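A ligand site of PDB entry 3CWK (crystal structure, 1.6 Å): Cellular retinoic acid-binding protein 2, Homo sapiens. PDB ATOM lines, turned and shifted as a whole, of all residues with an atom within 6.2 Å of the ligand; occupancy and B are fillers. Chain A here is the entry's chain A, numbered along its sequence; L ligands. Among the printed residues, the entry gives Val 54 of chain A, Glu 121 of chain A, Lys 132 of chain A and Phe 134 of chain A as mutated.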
ATOM      1  N   PHE A  15      20.513   7.554  -8.665  1.00  0.00           N
ATOM      2  CA  PHE A  15      21.429   8.641  -8.822  1.00  0.00           C
ATOM      3  C   PHE A  15      20.946   9.610  -9.855  1.00  0.00           C
ATOM      4  O   PHE A  15      21.118  10.804  -9.678  1.00  0.00           O
ATOM      5  CB  PHE A  15      22.782   8.063  -9.139  1.00  0.00           C
ATOM      6  CG  PHE A  15      23.881   9.056  -9.127  1.00  0.00           C
ATOM      7  CD1 PHE A  15      24.166   9.799  -8.017  1.00  0.00           C
ATOM      8  CD2 PHE A  15      24.702   9.169 -10.242  1.00  0.00           C
ATOM      9  CE1 PHE A  15      25.223  10.701  -8.005  1.00  0.00           C
ATOM     10  CE2 PHE A  15      25.773  10.072 -10.226  1.00  0.00           C
ATOM     11  CZ  PHE A  15      26.017  10.821  -9.110  1.00  0.00           C
ATOM     12  N   LEU A  19      20.380  13.789  -9.272  1.00  0.00           N
ATOM     13  CA  LEU A  19      20.989  14.825 -10.099  1.00  0.00           C
ATOM     14  C   LEU A  19      19.956  15.715 -10.748  1.00  0.00           C
ATOM     15  O   LEU A  19      20.191  16.922 -10.951  1.00  0.00           O
ATOM     16  CB  LEU A  19      21.897  14.214 -11.149  1.00  0.00           C
ATOM     17  CG  LEU A  19      23.080  13.387 -10.618  1.00  0.00           C
ATOM     18  CD1 LEU A  19      23.901  12.899 -11.773  1.00  0.00           C
ATOM     19  CD2 LEU A  19      23.872  14.177  -9.587  1.00  0.00           C
ATOM     20  N   VAL A  24      21.063  19.212 -12.637  1.00  0.00           N
ATOM     21  CA  VAL A  24      22.046  18.820 -13.614  1.00  0.00           C
ATOM     22  C   VAL A  24      21.345  18.462 -14.932  1.00  0.00           C
ATOM     23  O   VAL A  24      20.377  17.729 -14.918  1.00  0.00           O
ATOM     24  CB  VAL A  24      22.909  17.609 -13.122  1.00  0.00           C
ATOM     25  CG1 VAL A  24      23.913  17.222 -14.165  1.00  0.00           C
ATOM     26  CG2 VAL A  24      23.539  17.913 -11.818  1.00  0.00           C
ATOM     27  N   LEU A  28      24.855  15.948 -19.198  1.00  0.00           N
ATOM     28  CA  LEU A  28      25.786  15.759 -18.075  1.00  0.00           C
ATOM     29  C   LEU A  28      25.330  14.673 -17.171  1.00  0.00           C
ATOM     30  O   LEU A  28      26.151  13.929 -16.617  1.00  0.00           O
ATOM     31  CB  LEU A  28      25.914  17.024 -17.216  1.00  0.00           C
ATOM     32  CG  LEU A  28      26.819  18.098 -17.698  1.00  0.00           C
ATOM     33  CD1 LEU A  28      26.634  19.354 -16.842  1.00  0.00           C
ATOM     34  CD2 LEU A  28      28.273  17.606 -17.693  1.00  0.00           C
ATOM     35  N   ARG A  29      24.019  14.550 -16.983  1.00  0.00           N
ATOM     36  CA  ARG A  29      23.549  13.466 -16.108  1.00  0.00           C
ATOM     37  C   ARG A  29      23.924  12.137 -16.713  1.00  0.00           C
ATOM     38  O   ARG A  29      24.300  11.200 -16.009  1.00  0.00           O
ATOM     39  CB  ARG A  29      22.056  13.475 -15.874  1.00  0.00           C
ATOM     40  CG  ARG A  29      21.593  14.501 -15.016  1.00  0.00           C
ATOM     41  CD  ARG A  29      20.176  14.237 -14.543  1.00  0.00           C
ATOM     42  NE  ARG A  29      19.220  13.883 -15.584  1.00  0.00           N
ATOM     43  CZ  ARG A  29      18.372  14.726 -16.164  1.00  0.00           C
ATOM     44  NH1 ARG A  29      18.382  16.017 -15.918  1.00  0.00           N
ATOM     45  NH2 ARG A  29      17.476  14.245 -17.017  1.00  0.00           N
ATOM     46  N   ILE A  31      26.520  11.250 -18.563  1.00  0.00           N
ATOM     47  CA  ILE A  31      27.944  11.022 -18.243  1.00  0.00           C
ATOM     48  C   ILE A  31      28.120  10.613 -16.784  1.00  0.00           C
ATOM     49  O   ILE A  31      28.840   9.649 -16.457  1.00  0.00           O
ATOM     50  CB  ILE A  31      28.745  12.347 -18.483  1.00  0.00           C
ATOM     51  CG1 ILE A  31      28.692  12.740 -19.946  1.00  0.00           C
ATOM     52  CG2 ILE A  31      30.133  12.308 -17.946  1.00  0.00           C
ATOM     53  CD1 ILE A  31      29.253  14.165 -20.270  1.00  0.00           C
ATOM     54  N   ALA A  32      27.497  11.386 -15.889  1.00  0.00           N
ATOM     55  CA  ALA A  32      27.685  11.148 -14.465  1.00  0.00           C
ATOM     56  C   ALA A  32      27.193   9.780 -14.098  1.00  0.00           C
ATOM     57  O   ALA A  32      27.847   9.094 -13.334  1.00  0.00           O
ATOM     58  CB  ALA A  32      26.969  12.231 -13.637  1.00  0.00           C
ATOM     59  N   VAL A  33      26.009   9.421 -14.624  1.00  0.00           N
ATOM     60  CA  VAL A  33      25.381   8.163 -14.228  1.00  0.00           C
ATOM     61  C   VAL A  33      26.255   6.996 -14.682  1.00  0.00           C
ATOM     62  O   VAL A  33      26.501   6.062 -13.923  1.00  0.00           O
ATOM     63  CB  VAL A  33      23.942   8.083 -14.770  1.00  0.00           C
ATOM     64  CG1 VAL A  33      23.348   6.692 -14.564  1.00  0.00           C
ATOM     65  CG2 VAL A  33      23.058   9.126 -14.076  1.00  0.00           C
ATOM     66  N   ALA A  35      29.603   6.833 -15.214  1.00  0.00           N
ATOM     67  CA  ALA A  35      30.763   6.776 -14.338  1.00  0.00           C
ATOM     68  C   ALA A  35      30.516   6.397 -12.902  1.00  0.00           C
ATOM     69  O   ALA A  35      31.343   5.747 -12.244  1.00  0.00           O
ATOM     70  CB  ALA A  35      31.444   8.106 -14.397  1.00  0.00           C
ATOM     71  N   ALA A  36      29.363   6.772 -12.363  1.00  0.00           N
ATOM     72  CA  ALA A  36      29.120   6.526 -10.949  1.00  0.00           C
ATOM     73  C   ALA A  36      28.675   5.073 -10.761  1.00  0.00           C
ATOM     74  O   ALA A  36      28.477   4.676  -9.632  1.00  0.00           O
ATOM     75  CB  ALA A  36      28.096   7.503 -10.395  1.00  0.00           C
ATOM     76  N   PRO A  39      32.074   3.145  -8.712  1.00  0.00           N
ATOM     77  CA  PRO A  39      32.938   3.972  -7.873  1.00  0.00           C
ATOM     78  C   PRO A  39      33.705   3.117  -6.925  1.00  0.00           C
ATOM     79  O   PRO A  39      33.137   2.169  -6.376  1.00  0.00           O
ATOM     80  CB  PRO A  39      31.948   4.785  -7.038  1.00  0.00           C
ATOM     81  CG  PRO A  39      30.704   4.018  -7.011  1.00  0.00           C
ATOM     82  CD  PRO A  39      30.692   3.116  -8.207  1.00  0.00           C
ATOM     83  N   VAL A  41      35.487   3.283  -3.264  1.00  0.00           N
ATOM     84  CA  VAL A  41      35.428   4.111  -2.053  1.00  0.00           C
ATOM     85  C   VAL A  41      36.441   3.576  -1.068  1.00  0.00           C
ATOM     86  O   VAL A  41      36.378   2.392  -0.688  1.00  0.00           O
ATOM     87  CB  VAL A  41      34.047   4.076  -1.433  1.00  0.00           C
ATOM     88  CG1 VAL A  41      33.998   4.841  -0.113  1.00  0.00           C
ATOM     89  CG2 VAL A  41      33.051   4.670  -2.403  1.00  0.00           C
ATOM     90  N   ILE A  52      38.086   9.883   3.576  1.00  0.00           N
ATOM     91  CA  ILE A  52      37.309   9.157   2.589  1.00  0.00           C
ATOM     92  C   ILE A  52      37.645   9.629   1.212  1.00  0.00           C
ATOM     93  O   ILE A  52      37.558  10.848   0.956  1.00  0.00           O
ATOM     94  CB  ILE A  52      35.787   9.372   2.808  1.00  0.00           C
ATOM     95  CG1 ILE A  52      35.407   9.038   4.240  1.00  0.00           C
ATOM     96  CG2 ILE A  52      35.011   8.576   1.775  1.00  0.00           C
ATOM     97  CD1 ILE A  52      33.937   9.087   4.502  1.00  0.00           C
ATOM     98  N   VAL A  54      36.663   8.906  -2.844  1.00  0.00           N
ATOM     99  CA  VAL A  54      35.725   8.318  -3.783  1.00  0.00           C
ATOM    100  C   VAL A  54      36.271   8.530  -5.193  1.00  0.00           C
ATOM    101  O   VAL A  54      36.508   9.678  -5.544  1.00  0.00           O
ATOM    102  CB  VAL A  54      34.333   8.919  -3.677  1.00  0.00           C
ATOM    103  CG1 VAL A  54      33.417   8.294  -4.715  1.00  0.00           C
ATOM    104  CG2 VAL A  54      33.838   8.734  -2.225  1.00  0.00           C
ATOM    105  N   THR A  56      35.881   7.785  -9.383  1.00  0.00           N
ATOM    106  CA  THR A  56      35.198   7.375 -10.620  1.00  0.00           C
ATOM    107  C   THR A  56      36.027   7.888 -11.753  1.00  0.00           C
ATOM    108  O   THR A  56      36.900   8.712 -11.513  1.00  0.00           O
ATOM    109  CB  THR A  56      33.787   7.911 -10.754  1.00  0.00           C
ATOM    110  OG1 THR A  56      33.806   9.316 -10.948  1.00  0.00           O
ATOM    111  CG2 THR A  56      32.986   7.631  -9.520  1.00  0.00           C
ATOM    112  N   VAL A  58      35.281  10.105 -13.849  1.00  0.00           N
ATOM    113  CA  VAL A  58      34.998  11.508 -14.103  1.00  0.00           C
ATOM    114  C   VAL A  58      35.097  12.439 -12.866  1.00  0.00           C
ATOM    115  O   VAL A  58      34.960  13.662 -12.992  1.00  0.00           O
ATOM    116  CB  VAL A  58      33.582  11.705 -14.732  1.00  0.00           C
ATOM    117  CG1 VAL A  58      33.463  10.917 -16.034  1.00  0.00           C
ATOM    118  CG2 VAL A  58      32.493  11.329 -13.795  1.00  0.00           C
ATOM    119  N   ARG A  59      35.345  11.853 -11.697  1.00  0.00           N
ATOM    120  CA  ARG A  59      35.461  12.667 -10.485  1.00  0.00           C
ATOM    121  C   ARG A  59      36.059  11.840  -9.377  1.00  0.00           C
ATOM    122  O   ARG A  59      35.587  10.744  -9.110  1.00  0.00           O
ATOM    123  CB  ARG A  59      34.158  13.275 -10.059  1.00  0.00           C
ATOM    124  CG  ARG A  59      34.375  14.184  -8.877  1.00  0.00           C
ATOM    125  CD  ARG A  59      33.152  14.511  -8.216  1.00  0.00           C
ATOM    126  NE  ARG A  59      32.465  15.571  -8.891  1.00  0.00           N
ATOM    127  CZ  ARG A  59      31.223  15.938  -8.581  1.00  0.00           C
ATOM    128  NH1 ARG A  59      30.593  15.252  -7.643  1.00  0.00           N
ATOM    129  NH2 ARG A  59      30.602  16.940  -9.250  1.00  0.00           N
ATOM    130  N   THR A  61      37.214  12.510  -5.232  1.00  0.00           N
ATOM    131  CA  THR A  61      37.126  13.421  -4.080  1.00  0.00           C
ATOM    132  C   THR A  61      37.849  12.771  -2.939  1.00  0.00           C
ATOM    133  O   THR A  61      37.909  11.546  -2.850  1.00  0.00           O
ATOM    134  CB  THR A  61      35.744  13.751  -3.646  1.00  0.00           C
ATOM    135  OG1 THR A  61      35.005  12.569  -3.305  1.00  0.00           O
ATOM    136  CG2 THR A  61      34.988  14.498  -4.743  1.00  0.00           C
ATOM    137  N   VAL A  76      27.315  17.014  -4.232  1.00  0.00           N
ATOM    138  CA  VAL A  76      27.583  16.056  -5.299  1.00  0.00           C
ATOM    139  C   VAL A  76      27.544  16.713  -6.676  1.00  0.00           C
ATOM    140  O   VAL A  76      28.245  16.267  -7.594  1.00  0.00           O
ATOM    141  CB  VAL A  76      26.645  14.828  -5.297  1.00  0.00           C
ATOM    142  CG1 VAL A  76      27.383  13.617  -5.937  1.00  0.00           C
ATOM    143  CG2 VAL A  76      26.226  14.457  -3.959  1.00  0.00           C
ATOM    144  N   ASP A  77      26.808  17.796  -6.819  1.00  0.00           N
ATOM    145  CA  ASP A  77      26.808  18.530  -8.070  1.00  0.00           C
ATOM    146  C   ASP A  77      27.909  19.595  -8.120  1.00  0.00           C
ATOM    147  O   ASP A  77      27.988  20.426  -9.055  1.00  0.00           O
ATOM    148  CB  ASP A  77      25.441  19.120  -8.382  1.00  0.00           C
ATOM    149  CG  ASP A  77      25.008  20.144  -7.364  1.00  0.00           C
ATOM    150  OD1 ASP A  77      25.029  19.816  -6.150  1.00  0.00           O
ATOM    151  OD2 ASP A  77      24.584  21.238  -7.777  1.00  0.00           O
ATOM    152  N   GLY A  78      28.802  19.575  -7.127  1.00  0.00           N
ATOM    153  CA  GLY A  78      30.009  20.365  -7.116  1.00  0.00           C
ATOM    154  C   GLY A  78      29.964  21.764  -6.584  1.00  0.00           C
ATOM    155  O   GLY A  78      30.884  22.512  -6.873  1.00  0.00           O
ATOM    156  N   GLU A 121      25.566   3.774   1.671  1.00  0.00           N
ATOM    157  CA  GLU A 121      25.720   5.230   1.548  1.00  0.00           C
ATOM    158  C   GLU A 121      24.427   5.811   1.035  1.00  0.00           C
ATOM    159  O   GLU A 121      23.829   5.247   0.127  1.00  0.00           O
ATOM    160  CB  GLU A 121      26.796   5.555   0.532  1.00  0.00           C
ATOM    161  CG  GLU A 121      26.938   7.069   0.287  1.00  0.00           C
ATOM    162  CD  GLU A 121      28.156   7.435  -0.536  1.00  0.00           C
ATOM    163  OE1 GLU A 121      28.637   8.567  -0.386  1.00  0.00           O
ATOM    164  OE2 GLU A 121      28.658   6.594  -1.310  1.00  0.00           O
ATOM    165  N   MET A 123      22.794   9.710  -0.400  1.00  0.00           N
ATOM    166  CA  MET A 123      22.922  11.143  -0.685  1.00  0.00           C
ATOM    167  C   MET A 123      21.540  11.693  -0.912  1.00  0.00           C
ATOM    168  O   MET A 123      20.779  11.046  -1.610  1.00  0.00           O
ATOM    169  CB  MET A 123      23.760  11.314  -1.943  1.00  0.00           C
ATOM    170  CG  MET A 123      25.164  10.834  -1.765  1.00  0.00           C
ATOM    171  SD  MET A 123      26.109  10.981  -3.295  1.00  0.00           S
ATOM    172  CE  MET A 123      25.276   9.888  -4.265  1.00  0.00           C
ATOM    173  N   LYS A 132      23.505   3.679  -2.335  1.00  0.00           N
ATOM    174  CA  LYS A 132      24.570   2.806  -2.870  1.00  0.00           C
ATOM    175  C   LYS A 132      24.984   1.840  -1.785  1.00  0.00           C
ATOM    176  O   LYS A 132      25.003   2.205  -0.606  1.00  0.00           O
ATOM    177  CB  LYS A 132      25.748   3.624  -3.377  1.00  0.00           C
ATOM    178  CG  LYS A 132      25.388   4.422  -4.630  1.00  0.00           C
ATOM    179  CD  LYS A 132      26.494   5.337  -5.093  1.00  0.00           C
ATOM    180  CE  LYS A 132      26.172   6.685  -4.452  1.00  0.00           C
ATOM    181  NZ  LYS A 132      27.096   7.774  -4.678  1.00  0.00           N
ATOM    182  N   PHE A 134      27.920  -1.201  -0.706  1.00  0.00           N
ATOM    183  CA  PHE A 134      29.261  -1.708  -0.968  1.00  0.00           C
ATOM    184  C   PHE A 134      29.620  -2.880  -0.070  1.00  0.00           C
ATOM    185  O   PHE A 134      29.069  -3.022   1.008  1.00  0.00           O
ATOM    186  CB  PHE A 134      30.275  -0.619  -0.668  1.00  0.00           C
ATOM    187  CG  PHE A 134      30.091   0.678  -1.436  1.00  0.00           C
ATOM    188  CD1 PHE A 134      29.149   1.655  -1.020  1.00  0.00           C
ATOM    189  CD2 PHE A 134      30.858   0.939  -2.536  1.00  0.00           C
ATOM    190  CE1 PHE A 134      28.977   2.857  -1.723  1.00  0.00           C
ATOM    191  CE2 PHE A 134      30.668   2.135  -3.203  1.00  0.00           C
ATOM    192  CZ  PHE A 134      29.743   3.061  -2.796  1.00  0.00           C
HETATM  193  C1  LIG L   1      30.135  15.346 -13.513  1.00  0.00           C
HETATM  194  C2  LIG L   1      29.897  16.866 -13.746  1.00  0.00           C
HETATM  195  C3  LIG L   1      28.412  17.275 -13.741  1.00  0.00           C
HETATM  196  C4  LIG L   1      27.749  16.938 -12.448  1.00  0.00           C
HETATM  197  C5  LIG L   1      28.140  15.558 -11.958  1.00  0.00           C
HETATM  198  C6  LIG L   1      29.242  14.850 -12.418  1.00  0.00           C
HETATM  199  C7  LIG L   1      29.576  13.487 -11.945  1.00  0.00           C
HETATM  200  C8  LIG L   1      29.611  13.134 -10.583  1.00  0.00           C
HETATM  201  C9  LIG L   1      29.836  11.778 -10.120  1.00  0.00           C
HETATM  202  C10 LIG L   1      29.696  11.619  -8.687  1.00  0.00           C
HETATM  203  C11 LIG L   1      29.943  10.354  -8.055  1.00  0.00           C
HETATM  204  C12 LIG L   1      29.764  10.416  -6.609  1.00  0.00           C
HETATM  205  C13 LIG L   1      29.868   9.261  -5.810  1.00  0.00           C
HETATM  206  C14 LIG L   1      29.859   9.561  -4.431  1.00  0.00           C
HETATM  207  C15 LIG L   1      29.870   8.567  -3.385  1.00  0.00           C
HETATM  208  C16 LIG L   1      31.584  15.066 -13.091  1.00  0.00           C
HETATM  209  C17 LIG L   1      29.865  14.492 -14.764  1.00  0.00           C
HETATM  210  C18 LIG L   1      27.213  15.017 -10.925  1.00  0.00           C
HETATM  211  C19 LIG L   1      30.196  10.673 -11.045  1.00  0.00           C
HETATM  212  C20 LIG L   1      29.996   7.940  -6.445  1.00  0.00           C
HETATM  213  O1  LIG L   1      29.394   7.417  -3.614  1.00  0.00           O
HETATM  214  O2  LIG L   1      30.356   8.937  -2.262  1.00  0.00           O
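The side-chain carboxylate of Glu 121 is in salt-bridge range of the side-chain amino group of Lys 132 (3.9 Å).
The side-chain amino group (NZ) of Lys 132 lies close to the side-chain sulfur (SD) of Met 123, 3.6 Å away.
The backbone NH of Val 54 sits at hydrogen-bond distance from the backbone carbonyl oxygen of Thr 61 (2.9 Å).
OG1 of Thr 56 lies close to N of Val 58, at 3.3 Å.
The backbone NH (N) of Val 24 lies within hydrogen-bond range of the backbone carbonyl oxygen (O) of Leu 19 (3.0 Å).
NH1 of Arg 59 is in hydrogen-bond range of O of Val 76 (2.6 Å).
O of Arg 59 lies within hydrogen-bond range of OG1 of Thr 56 (2.9 Å).
Merely in contact with the ligand: Phe 15 (3.8 Å), Leu 19 (3.7 Å), Leu 28 (3.97 Å), Ile 31 (3.9 Å), Ala 32 (3.4 Å), Ala 36 (3.9 Å), Pro 39 (3.8 Å), Val 54 (3.5 Å), Thr 56 (3.9 Å), Val 58 (3.6 Å), Arg 59 (3.8 Å) and Val 76 (3.7 Å).
Hydrophobic or aromatic side chains that line the ligand: Phe 15, Leu 19, Leu 28, Ile 31, Ala 32, Ala 36, Pro 39, Val 54 and Val 58.
The nearest printed residue that does not touch the ligand is Met 123 (4.2 Å).
OE2 of Glu 121 lies close to O1 of the ligand (2.6 Å).
An oxygen (O1) of the ligand lies within salt-bridge range of the side-chain amino group (NZ) of Lys 132.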
